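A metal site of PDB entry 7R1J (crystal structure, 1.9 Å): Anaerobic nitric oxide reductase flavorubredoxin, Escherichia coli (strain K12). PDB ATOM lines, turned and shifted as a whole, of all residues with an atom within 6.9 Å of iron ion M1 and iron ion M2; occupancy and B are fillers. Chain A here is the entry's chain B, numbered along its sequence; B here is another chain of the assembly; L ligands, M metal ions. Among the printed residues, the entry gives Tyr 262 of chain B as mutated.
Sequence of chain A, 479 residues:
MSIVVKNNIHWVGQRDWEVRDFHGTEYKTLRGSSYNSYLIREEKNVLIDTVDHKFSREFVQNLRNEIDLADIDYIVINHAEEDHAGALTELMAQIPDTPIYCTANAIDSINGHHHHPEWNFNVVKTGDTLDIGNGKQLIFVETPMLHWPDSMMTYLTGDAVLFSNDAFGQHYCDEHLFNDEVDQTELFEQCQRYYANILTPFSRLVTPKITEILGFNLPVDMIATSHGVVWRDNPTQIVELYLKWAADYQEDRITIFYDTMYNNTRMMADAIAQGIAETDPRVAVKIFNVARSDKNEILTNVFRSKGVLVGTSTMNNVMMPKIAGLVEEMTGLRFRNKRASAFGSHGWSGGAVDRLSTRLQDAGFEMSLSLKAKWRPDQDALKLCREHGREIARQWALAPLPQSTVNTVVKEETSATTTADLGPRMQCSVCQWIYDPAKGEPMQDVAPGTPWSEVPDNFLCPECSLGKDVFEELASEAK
An oxygen (O1) of LG2 L2 lies within hydrogen-bond range of the side-chain hydroxyl (OH) of Tyr 194, 2.7 Å away. N of Tyr 262 of chain B sits at hydrogen-bond distance from O9 of LG3 L3, 2.7 Å away. A ring nitrogen (NE2) of His 147 sits close to an oxygen (O1) of LG2 L2, 3.2 Å away.
N of His 147 is in hydrogen-bond range of OG of Ser 151 (3.4 Å). The side-chain carboxylate (OD1) of Asp 166 lies close to the side-chain amide oxygen (OD1) of Asn 165. NE2 of His 23 lies within hydrogen-bond range of OE2 of Glu 81, 3.0 Å away. The side-chain hydroxyl (OG) of Ser 226 sits at hydrogen-bond distance from the backbone NH (N) of Asp 166, at 3.1 Å.
Within 4 Å of iron ion M1: His 79, Glu 81, His 147 and Asp 166.
Of the 18 residues printed, 4 come within 4 Å of iron ion M2.
OE1 of Glu 81 is bound to iron ion M1, at 1.8 Å. OD2 of Asp 166 binds iron ion M1 (2.1 Å). Iron ion M1 is bound by O1 of LIG L1 (2.4 Å). NE2 of His 147 is bound to iron ion M1, 2.4 Å away. NE2 of His 79 binds iron ion M1 (2.5 Å). Iron ion M1 has five donor atoms within binding distance.
Iron ion M2 is bound by an oxygen (O1) of LIG L1 (1.8 Å), a ring nitrogen (NE2) of His 84 (2.1 Å), a ring nitrogen (NE2) of His 227 (2.2 Å), the side-chain carboxylate of Asp 166 (2.4 Å) and the side-chain carboxylate of Asp 83 (2.4 Å).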
ATOM      1  N   PHE A  22       2.872  -5.266 -20.136  1.00  0.00           N
ATOM      2  CA  PHE A  22       3.455  -4.111 -19.453  1.00  0.00           C
ATOM      3  C   PHE A  22       4.505  -4.559 -18.450  1.00  0.00           C
ATOM      4  O   PHE A  22       4.371  -5.641 -17.849  1.00  0.00           O
ATOM      5  CB  PHE A  22       2.374  -3.278 -18.759  1.00  0.00           C
ATOM      6  CG  PHE A  22       1.952  -2.068 -19.536  1.00  0.00           C
ATOM      7  CD1 PHE A  22       1.022  -2.154 -20.553  1.00  0.00           C
ATOM      8  CD2 PHE A  22       2.477  -0.819 -19.223  1.00  0.00           C
ATOM      9  CE1 PHE A  22       0.630  -1.041 -21.260  1.00  0.00           C
ATOM     10  CE2 PHE A  22       2.092   0.304 -19.935  1.00  0.00           C
ATOM     11  CZ  PHE A  22       1.164   0.199 -20.951  1.00  0.00           C
ATOM     12  N   HIS A  23       5.533  -3.742 -18.250  1.00  0.00           N
ATOM     13  CA  HIS A  23       6.631  -4.050 -17.337  1.00  0.00           C
ATOM     14  C   HIS A  23       7.239  -5.413 -17.643  1.00  0.00           C
ATOM     15  O   HIS A  23       7.260  -6.306 -16.785  1.00  0.00           O
ATOM     16  CB  HIS A  23       6.156  -4.023 -15.886  1.00  0.00           C
ATOM     17  CG  HIS A  23       5.654  -2.678 -15.441  1.00  0.00           C
ATOM     18  ND1 HIS A  23       4.791  -2.529 -14.385  1.00  0.00           N
ATOM     19  CD2 HIS A  23       5.899  -1.434 -15.918  1.00  0.00           C
ATOM     20  CE1 HIS A  23       4.515  -1.249 -14.230  1.00  0.00           C
ATOM     21  NE2 HIS A  23       5.175  -0.563 -15.138  1.00  0.00           N
ATOM     22  N   TYR A  35      -2.401   6.198 -23.681  1.00  0.00           N
ATOM     23  CA  TYR A  35      -1.395   7.056 -23.103  1.00  0.00           C
ATOM     24  C   TYR A  35      -1.863   8.483 -23.265  1.00  0.00           C
ATOM     25  O   TYR A  35      -1.862   9.018 -24.379  1.00  0.00           O
ATOM     26  CB  TYR A  35      -0.036   6.823 -23.764  1.00  0.00           C
ATOM     27  CG  TYR A  35       0.244   5.352 -23.953  1.00  0.00           C
ATOM     28  CD1 TYR A  35       0.561   4.547 -22.858  1.00  0.00           C
ATOM     29  CD2 TYR A  35       0.162   4.753 -25.208  1.00  0.00           C
ATOM     30  CE1 TYR A  35       0.797   3.194 -23.010  1.00  0.00           C
ATOM     31  CE2 TYR A  35       0.408   3.400 -25.365  1.00  0.00           C
ATOM     32  CZ  TYR A  35       0.723   2.625 -24.271  1.00  0.00           C
ATOM     33  OH  TYR A  35       0.964   1.273 -24.414  1.00  0.00           O
ATOM     34  N   HIS A  79       5.749  12.493 -14.464  1.00  0.00           N
ATOM     35  CA  HIS A  79       6.286  11.174 -14.198  1.00  0.00           C
ATOM     36  C   HIS A  79       7.047  10.723 -15.418  1.00  0.00           C
ATOM     37  O   HIS A  79       6.505  10.720 -16.524  1.00  0.00           O
ATOM     38  CB  HIS A  79       5.147  10.218 -13.838  1.00  0.00           C
ATOM     39  CG  HIS A  79       5.552   8.785 -13.711  1.00  0.00           C
ATOM     40  ND1 HIS A  79       6.739   8.392 -13.140  1.00  0.00           N
ATOM     41  CD2 HIS A  79       4.898   7.657 -14.068  1.00  0.00           C
ATOM     42  CE1 HIS A  79       6.808   7.072 -13.154  1.00  0.00           C
ATOM     43  NE2 HIS A  79       5.706   6.599 -13.709  1.00  0.00           N
ATOM     44  N   GLU A  81       8.250   7.853 -16.665  1.00  0.00           N
ATOM     45  CA  GLU A  81       8.286   6.449 -17.038  1.00  0.00           C
ATOM     46  C   GLU A  81       8.193   6.332 -18.555  1.00  0.00           C
ATOM     47  O   GLU A  81       7.611   7.194 -19.217  1.00  0.00           O
ATOM     48  CB  GLU A  81       7.154   5.684 -16.358  1.00  0.00           C
ATOM     49  CG  GLU A  81       7.254   4.164 -16.441  1.00  0.00           C
ATOM     50  CD  GLU A  81       6.335   3.474 -15.446  1.00  0.00           C
ATOM     51  OE1 GLU A  81       5.617   4.173 -14.714  1.00  0.00           O
ATOM     52  OE2 GLU A  81       6.320   2.221 -15.422  1.00  0.00           O
ATOM     53  N   ASP A  83       6.352   4.937 -20.628  1.00  0.00           N
ATOM     54  CA  ASP A  83       5.050   5.029 -21.278  1.00  0.00           C
ATOM     55  C   ASP A  83       4.451   6.426 -21.192  1.00  0.00           C
ATOM     56  O   ASP A  83       3.309   6.637 -21.605  1.00  0.00           O
ATOM     57  CB  ASP A  83       4.077   4.012 -20.661  1.00  0.00           C
ATOM     58  CG  ASP A  83       3.878   4.219 -19.182  1.00  0.00           C
ATOM     59  OD1 ASP A  83       4.814   4.705 -18.509  1.00  0.00           O
ATOM     60  OD2 ASP A  83       2.783   3.892 -18.673  1.00  0.00           O
ATOM     61  N   HIS A  84       5.218   7.367 -20.655  1.00  0.00           N
ATOM     62  CA  HIS A  84       4.768   8.754 -20.566  1.00  0.00           C
ATOM     63  C   HIS A  84       5.853   9.712 -21.056  1.00  0.00           C
ATOM     64  O   HIS A  84       5.560  10.833 -21.454  1.00  0.00           O
ATOM     65  CB  HIS A  84       4.384   9.098 -19.125  1.00  0.00           C
ATOM     66  CG  HIS A  84       3.430   8.132 -18.511  1.00  0.00           C
ATOM     67  ND1 HIS A  84       2.221   7.792 -19.088  1.00  0.00           N
ATOM     68  CD2 HIS A  84       3.504   7.424 -17.355  1.00  0.00           C
ATOM     69  CE1 HIS A  84       1.599   6.914 -18.321  1.00  0.00           C
ATOM     70  NE2 HIS A  84       2.353   6.678 -17.261  1.00  0.00           N
ATOM     71  N   HIS A 147       3.404   6.524  -8.070  1.00  0.00           N
ATOM     72  CA  HIS A 147       4.025   5.342  -7.474  1.00  0.00           C
ATOM     73  C   HIS A 147       5.541   5.306  -7.678  1.00  0.00           C
ATOM     74  O   HIS A 147       6.196   4.306  -7.392  1.00  0.00           O
ATOM     75  CB  HIS A 147       3.401   4.068  -8.050  1.00  0.00           C
ATOM     76  CG  HIS A 147       3.589   3.911  -9.527  1.00  0.00           C
ATOM     77  ND1 HIS A 147       4.677   3.263 -10.079  1.00  0.00           N
ATOM     78  CD2 HIS A 147       2.837   4.327 -10.566  1.00  0.00           C
ATOM     79  CE1 HIS A 147       4.580   3.293 -11.390  1.00  0.00           C
ATOM     80  NE2 HIS A 147       3.473   3.930 -11.715  1.00  0.00           N
ATOM     81  N   TRP A 148       6.091   6.408  -8.188  1.00  0.00           N
ATOM     82  CA  TRP A 148       7.547   6.540  -8.361  1.00  0.00           C
ATOM     83  C   TRP A 148       8.071   7.725  -7.549  1.00  0.00           C
ATOM     84  O   TRP A 148       7.294   8.599  -7.158  1.00  0.00           O
ATOM     85  CB  TRP A 148       7.905   6.724  -9.846  1.00  0.00           C
ATOM     86  CG  TRP A 148       8.250   5.430 -10.551  1.00  0.00           C
ATOM     87  CD1 TRP A 148       7.833   4.180 -10.211  1.00  0.00           C
ATOM     88  CD2 TRP A 148       9.080   5.276 -11.713  1.00  0.00           C
ATOM     89  NE1 TRP A 148       8.354   3.253 -11.086  1.00  0.00           N
ATOM     90  CE2 TRP A 148       9.120   3.905 -12.012  1.00  0.00           C
ATOM     91  CE3 TRP A 148       9.795   6.169 -12.517  1.00  0.00           C
ATOM     92  CZ2 TRP A 148       9.848   3.406 -13.100  1.00  0.00           C
ATOM     93  CZ3 TRP A 148      10.506   5.669 -13.596  1.00  0.00           C
ATOM     94  CH2 TRP A 148      10.532   4.297 -13.876  1.00  0.00           C
ATOM     95  N   SER A 151       7.083  11.085  -9.138  1.00  0.00           N
ATOM     96  CA  SER A 151       5.671  11.322  -9.439  1.00  0.00           C
ATOM     97  C   SER A 151       5.133  12.611  -8.826  1.00  0.00           C
ATOM     98  O   SER A 151       5.467  12.972  -7.695  1.00  0.00           O
ATOM     99  CB  SER A 151       4.825  10.139  -8.965  1.00  0.00           C
ATOM    100  OG  SER A 151       5.191   8.947  -9.643  1.00  0.00           O
ATOM    101  N   ASN A 165      -1.751  12.060 -13.681  1.00  0.00           N
ATOM    102  CA  ASN A 165      -0.877  11.046 -14.268  1.00  0.00           C
ATOM    103  C   ASN A 165      -1.395   9.629 -13.945  1.00  0.00           C
ATOM    104  O   ASN A 165      -2.571   9.363 -14.140  1.00  0.00           O
ATOM    105  CB  ASN A 165       0.571  11.229 -13.790  1.00  0.00           C
ATOM    106  CG  ASN A 165       1.573  10.484 -14.651  1.00  0.00           C
ATOM    107  OD1 ASN A 165       2.050   9.416 -14.260  1.00  0.00           O
ATOM    108  ND2 ASN A 165       1.896  11.028 -15.817  1.00  0.00           N
ATOM    109  N   ASP A 166      -0.530   8.740 -13.458  1.00  0.00           N
ATOM    110  CA  ASP A 166      -0.920   7.348 -13.212  1.00  0.00           C
ATOM    111  C   ASP A 166      -2.072   7.194 -12.226  1.00  0.00           C
ATOM    112  O   ASP A 166      -2.901   6.292 -12.374  1.00  0.00           O
ATOM    113  CB  ASP A 166       0.277   6.532 -12.708  1.00  0.00           C
ATOM    114  CG  ASP A 166       1.227   6.137 -13.814  1.00  0.00           C
ATOM    115  OD1 ASP A 166       0.856   6.264 -14.993  1.00  0.00           O
ATOM    116  OD2 ASP A 166       2.349   5.681 -13.486  1.00  0.00           O
ATOM    117  N   HIS A 171      -5.778   0.789 -17.386  1.00  0.00           N
ATOM    118  CA  HIS A 171      -5.467   0.333 -18.737  1.00  0.00           C
ATOM    119  C   HIS A 171      -6.734  -0.165 -19.421  1.00  0.00           C
ATOM    120  O   HIS A 171      -7.109  -1.329 -19.299  1.00  0.00           O
ATOM    121  CB  HIS A 171      -4.386  -0.757 -18.706  1.00  0.00           C
ATOM    122  CG  HIS A 171      -3.065  -0.272 -18.206  1.00  0.00           C
ATOM    123  ND1 HIS A 171      -2.337   0.708 -18.843  1.00  0.00           N
ATOM    124  CD2 HIS A 171      -2.353  -0.609 -17.107  1.00  0.00           C
ATOM    125  CE1 HIS A 171      -1.222   0.935 -18.176  1.00  0.00           C
ATOM    126  NE2 HIS A 171      -1.212   0.159 -17.107  1.00  0.00           N
ATOM    127  N   TYR A 194      -5.662  -2.498 -11.835  1.00  0.00           N
ATOM    128  CA  TYR A 194      -4.526  -1.590 -11.831  1.00  0.00           C
ATOM    129  C   TYR A 194      -4.050  -1.300 -10.407  1.00  0.00           C
ATOM    130  O   TYR A 194      -2.858  -1.402 -10.128  1.00  0.00           O
ATOM    131  CB  TYR A 194      -4.883  -0.273 -12.536  1.00  0.00           C
ATOM    132  CG  TYR A 194      -3.718   0.673 -12.650  1.00  0.00           C
ATOM    133  CD1 TYR A 194      -3.519   1.690 -11.719  1.00  0.00           C
ATOM    134  CD2 TYR A 194      -2.808   0.558 -13.698  1.00  0.00           C
ATOM    135  CE1 TYR A 194      -2.448   2.560 -11.826  1.00  0.00           C
ATOM    136  CE2 TYR A 194      -1.737   1.428 -13.805  1.00  0.00           C
ATOM    137  CZ  TYR A 194      -1.559   2.424 -12.873  1.00  0.00           C
ATOM    138  OH  TYR A 194      -0.482   3.273 -12.992  1.00  0.00           O
ATOM    139  N   ILE A 198      -0.342  -2.780  -8.962  1.00  0.00           N
ATOM    140  CA  ILE A 198       0.658  -1.724  -9.057  1.00  0.00           C
ATOM    141  C   ILE A 198       0.773  -0.872  -7.802  1.00  0.00           C
ATOM    142  O   ILE A 198       1.879  -0.612  -7.324  1.00  0.00           O
ATOM    143  CB  ILE A 198       0.359  -0.791 -10.259  1.00  0.00           C
ATOM    144  CG1 ILE A 198       0.322  -1.599 -11.556  1.00  0.00           C
ATOM    145  CG2 ILE A 198       1.405   0.319 -10.347  1.00  0.00           C
ATOM    146  CD1 ILE A 198       1.609  -2.315 -11.856  1.00  0.00           C
ATOM    147  N   SER A 226      -3.213   9.622 -16.830  1.00  0.00           N
ATOM    148  CA  SER A 226      -2.316   9.294 -17.925  1.00  0.00           C
ATOM    149  C   SER A 226      -2.748   8.017 -18.653  1.00  0.00           C
ATOM    150  O   SER A 226      -2.214   7.687 -19.710  1.00  0.00           O
ATOM    151  CB  SER A 226      -0.887   9.155 -17.426  1.00  0.00           C
ATOM    152  OG  SER A 226      -0.760   8.091 -16.509  1.00  0.00           O
ATOM    153  N   HIS A 227      -3.700   7.291 -18.078  1.00  0.00           N
ATOM    154  CA  HIS A 227      -4.186   6.046 -18.669  1.00  0.00           C
ATOM    155  C   HIS A 227      -5.708   5.945 -18.644  1.00  0.00           C
ATOM    156  O   HIS A 227      -6.324   6.090 -17.590  1.00  0.00           O
ATOM    157  CB  HIS A 227      -3.603   4.825 -17.950  1.00  0.00           C
ATOM    158  CG  HIS A 227      -2.126   4.646 -18.136  1.00  0.00           C
ATOM    159  ND1 HIS A 227      -1.550   4.403 -19.365  1.00  0.00           N
ATOM    160  CD2 HIS A 227      -1.113   4.663 -17.246  1.00  0.00           C
ATOM    161  CE1 HIS A 227      -0.251   4.293 -19.230  1.00  0.00           C
ATOM    162  NE2 HIS A 227       0.044   4.446 -17.952  1.00  0.00           N
ATOM    163  N   TYR B 262      12.350  -2.553 -19.042  1.00  0.00           N
ATOM    164  CA  TYR B 262      12.625  -1.463 -19.984  1.00  0.00           C
ATOM    165  C   TYR B 262      13.925  -1.684 -20.762  1.00  0.00           C
ATOM    166  O   TYR B 262      14.458  -0.735 -21.343  1.00  0.00           O
ATOM    167  CB  TYR B 262      12.696  -0.140 -19.233  1.00  0.00           C
ATOM    168  CG  TYR B 262      11.433   0.192 -18.481  1.00  0.00           C
ATOM    169  CD1 TYR B 262      10.220   0.290 -19.154  1.00  0.00           C
ATOM    170  CD2 TYR B 262      11.447   0.410 -17.110  1.00  0.00           C
ATOM    171  CE1 TYR B 262       9.063   0.586 -18.486  1.00  0.00           C
ATOM    172  CE2 TYR B 262      10.285   0.706 -16.429  1.00  0.00           C
ATOM    173  CZ  TYR B 262       9.095   0.794 -17.124  1.00  0.00           C
ATOM    174  OH  TYR B 262       7.933   1.090 -16.466  1.00  0.00           O
HETATM  175  O1  LIG L   1       3.507   4.605 -16.190  1.00  0.00           O
HETATM  176  O1  LG2 L   2       1.887   2.432 -14.090  1.00  0.00           O
HETATM  177  O2  LG2 L   2       2.392   2.338 -15.181  1.00  0.00           O
HETATM  178  N1  LG3 L   3      13.660   0.714  -8.527  1.00  0.00           N
HETATM  179  C1  LG3 L   3      14.149   0.578  -7.250  1.00  0.00           C
HETATM  180  O1  LG3 L   3      15.281   0.974  -6.974  1.00  0.00           O
HETATM  181  N2  LG3 L   3      13.365   0.008  -6.264  1.00  0.00           N
HETATM  182  C2  LG3 L   3      12.093  -0.438  -6.556  1.00  0.00           C
HETATM  183  O2  LG3 L   3      11.416  -0.944  -5.663  1.00  0.00           O
HETATM  184  C3  LG3 L   3      11.595  -0.314  -7.851  1.00  0.00           C
HETATM  185  N3  LG3 L   3      10.313  -0.750  -8.160  1.00  0.00           N
HETATM  186  C4  LG3 L   3       9.833  -0.615  -9.442  1.00  0.00           C
HETATM  187  C5  LG3 L   3       8.555  -1.051  -9.765  1.00  0.00           C
HETATM  188  C6  LG3 L   3       8.057  -0.917 -11.060  1.00  0.00           C
HETATM  189  C7  LG3 L   3       6.679  -1.392 -11.409  1.00  0.00           C
HETATM  190  C8  LG3 L   3       8.854  -0.335 -12.042  1.00  0.00           C
HETATM  191  C9  LG3 L   3       8.331  -0.187 -13.449  1.00  0.00           C
HETATM  192  C10 LG3 L   3      10.127   0.101 -11.728  1.00  0.00           C
HETATM  193  C11 LG3 L   3      10.625  -0.033 -10.432  1.00  0.00           C
HETATM  194  N4  LG3 L   3      11.898   0.403 -10.118  1.00  0.00           N
HETATM  195  C12 LG3 L   3      12.383   0.268  -8.827  1.00  0.00           C
HETATM  196  C13 LG3 L   3      12.776   1.038 -11.156  1.00  0.00           C
HETATM  197  C14 LG3 L   3      13.483   0.013 -12.028  1.00  0.00           C
HETATM  198  O3  LG3 L   3      14.323  -0.798 -11.254  1.00  0.00           O
HETATM  199  C15 LG3 L   3      14.285   0.773 -13.092  1.00  0.00           C
HETATM  200  O4  LG3 L   3      13.381   1.334 -14.019  1.00  0.00           O
HETATM  201  C16 LG3 L   3      15.255  -0.140 -13.836  1.00  0.00           C
HETATM  202  O5  LG3 L   3      16.164   0.669 -14.553  1.00  0.00           O
HETATM  203  C17 LG3 L   3      14.520  -1.063 -14.794  1.00  0.00           C
HETATM  204  O6  LG3 L   3      15.430  -2.003 -15.327  1.00  0.00           O
HETATM  205  P1  LG3 L   3      14.960  -3.026 -16.480  1.00  0.00           P
HETATM  206  O7  LG3 L   3      16.063  -4.004 -16.748  1.00  0.00           O
HETATM  207  O8  LG3 L   3      13.708  -3.756 -16.032  1.00  0.00           O
HETATM  208  O9  LG3 L   3      14.676  -2.265 -17.757  1.00  0.00           O
HETATM  209 FE    FE M   1       4.138   4.673 -13.909  1.00  0.00          FE
HETATM  210 FE    FE M   2       1.787   4.737 -16.620  1.00  0.00          FE
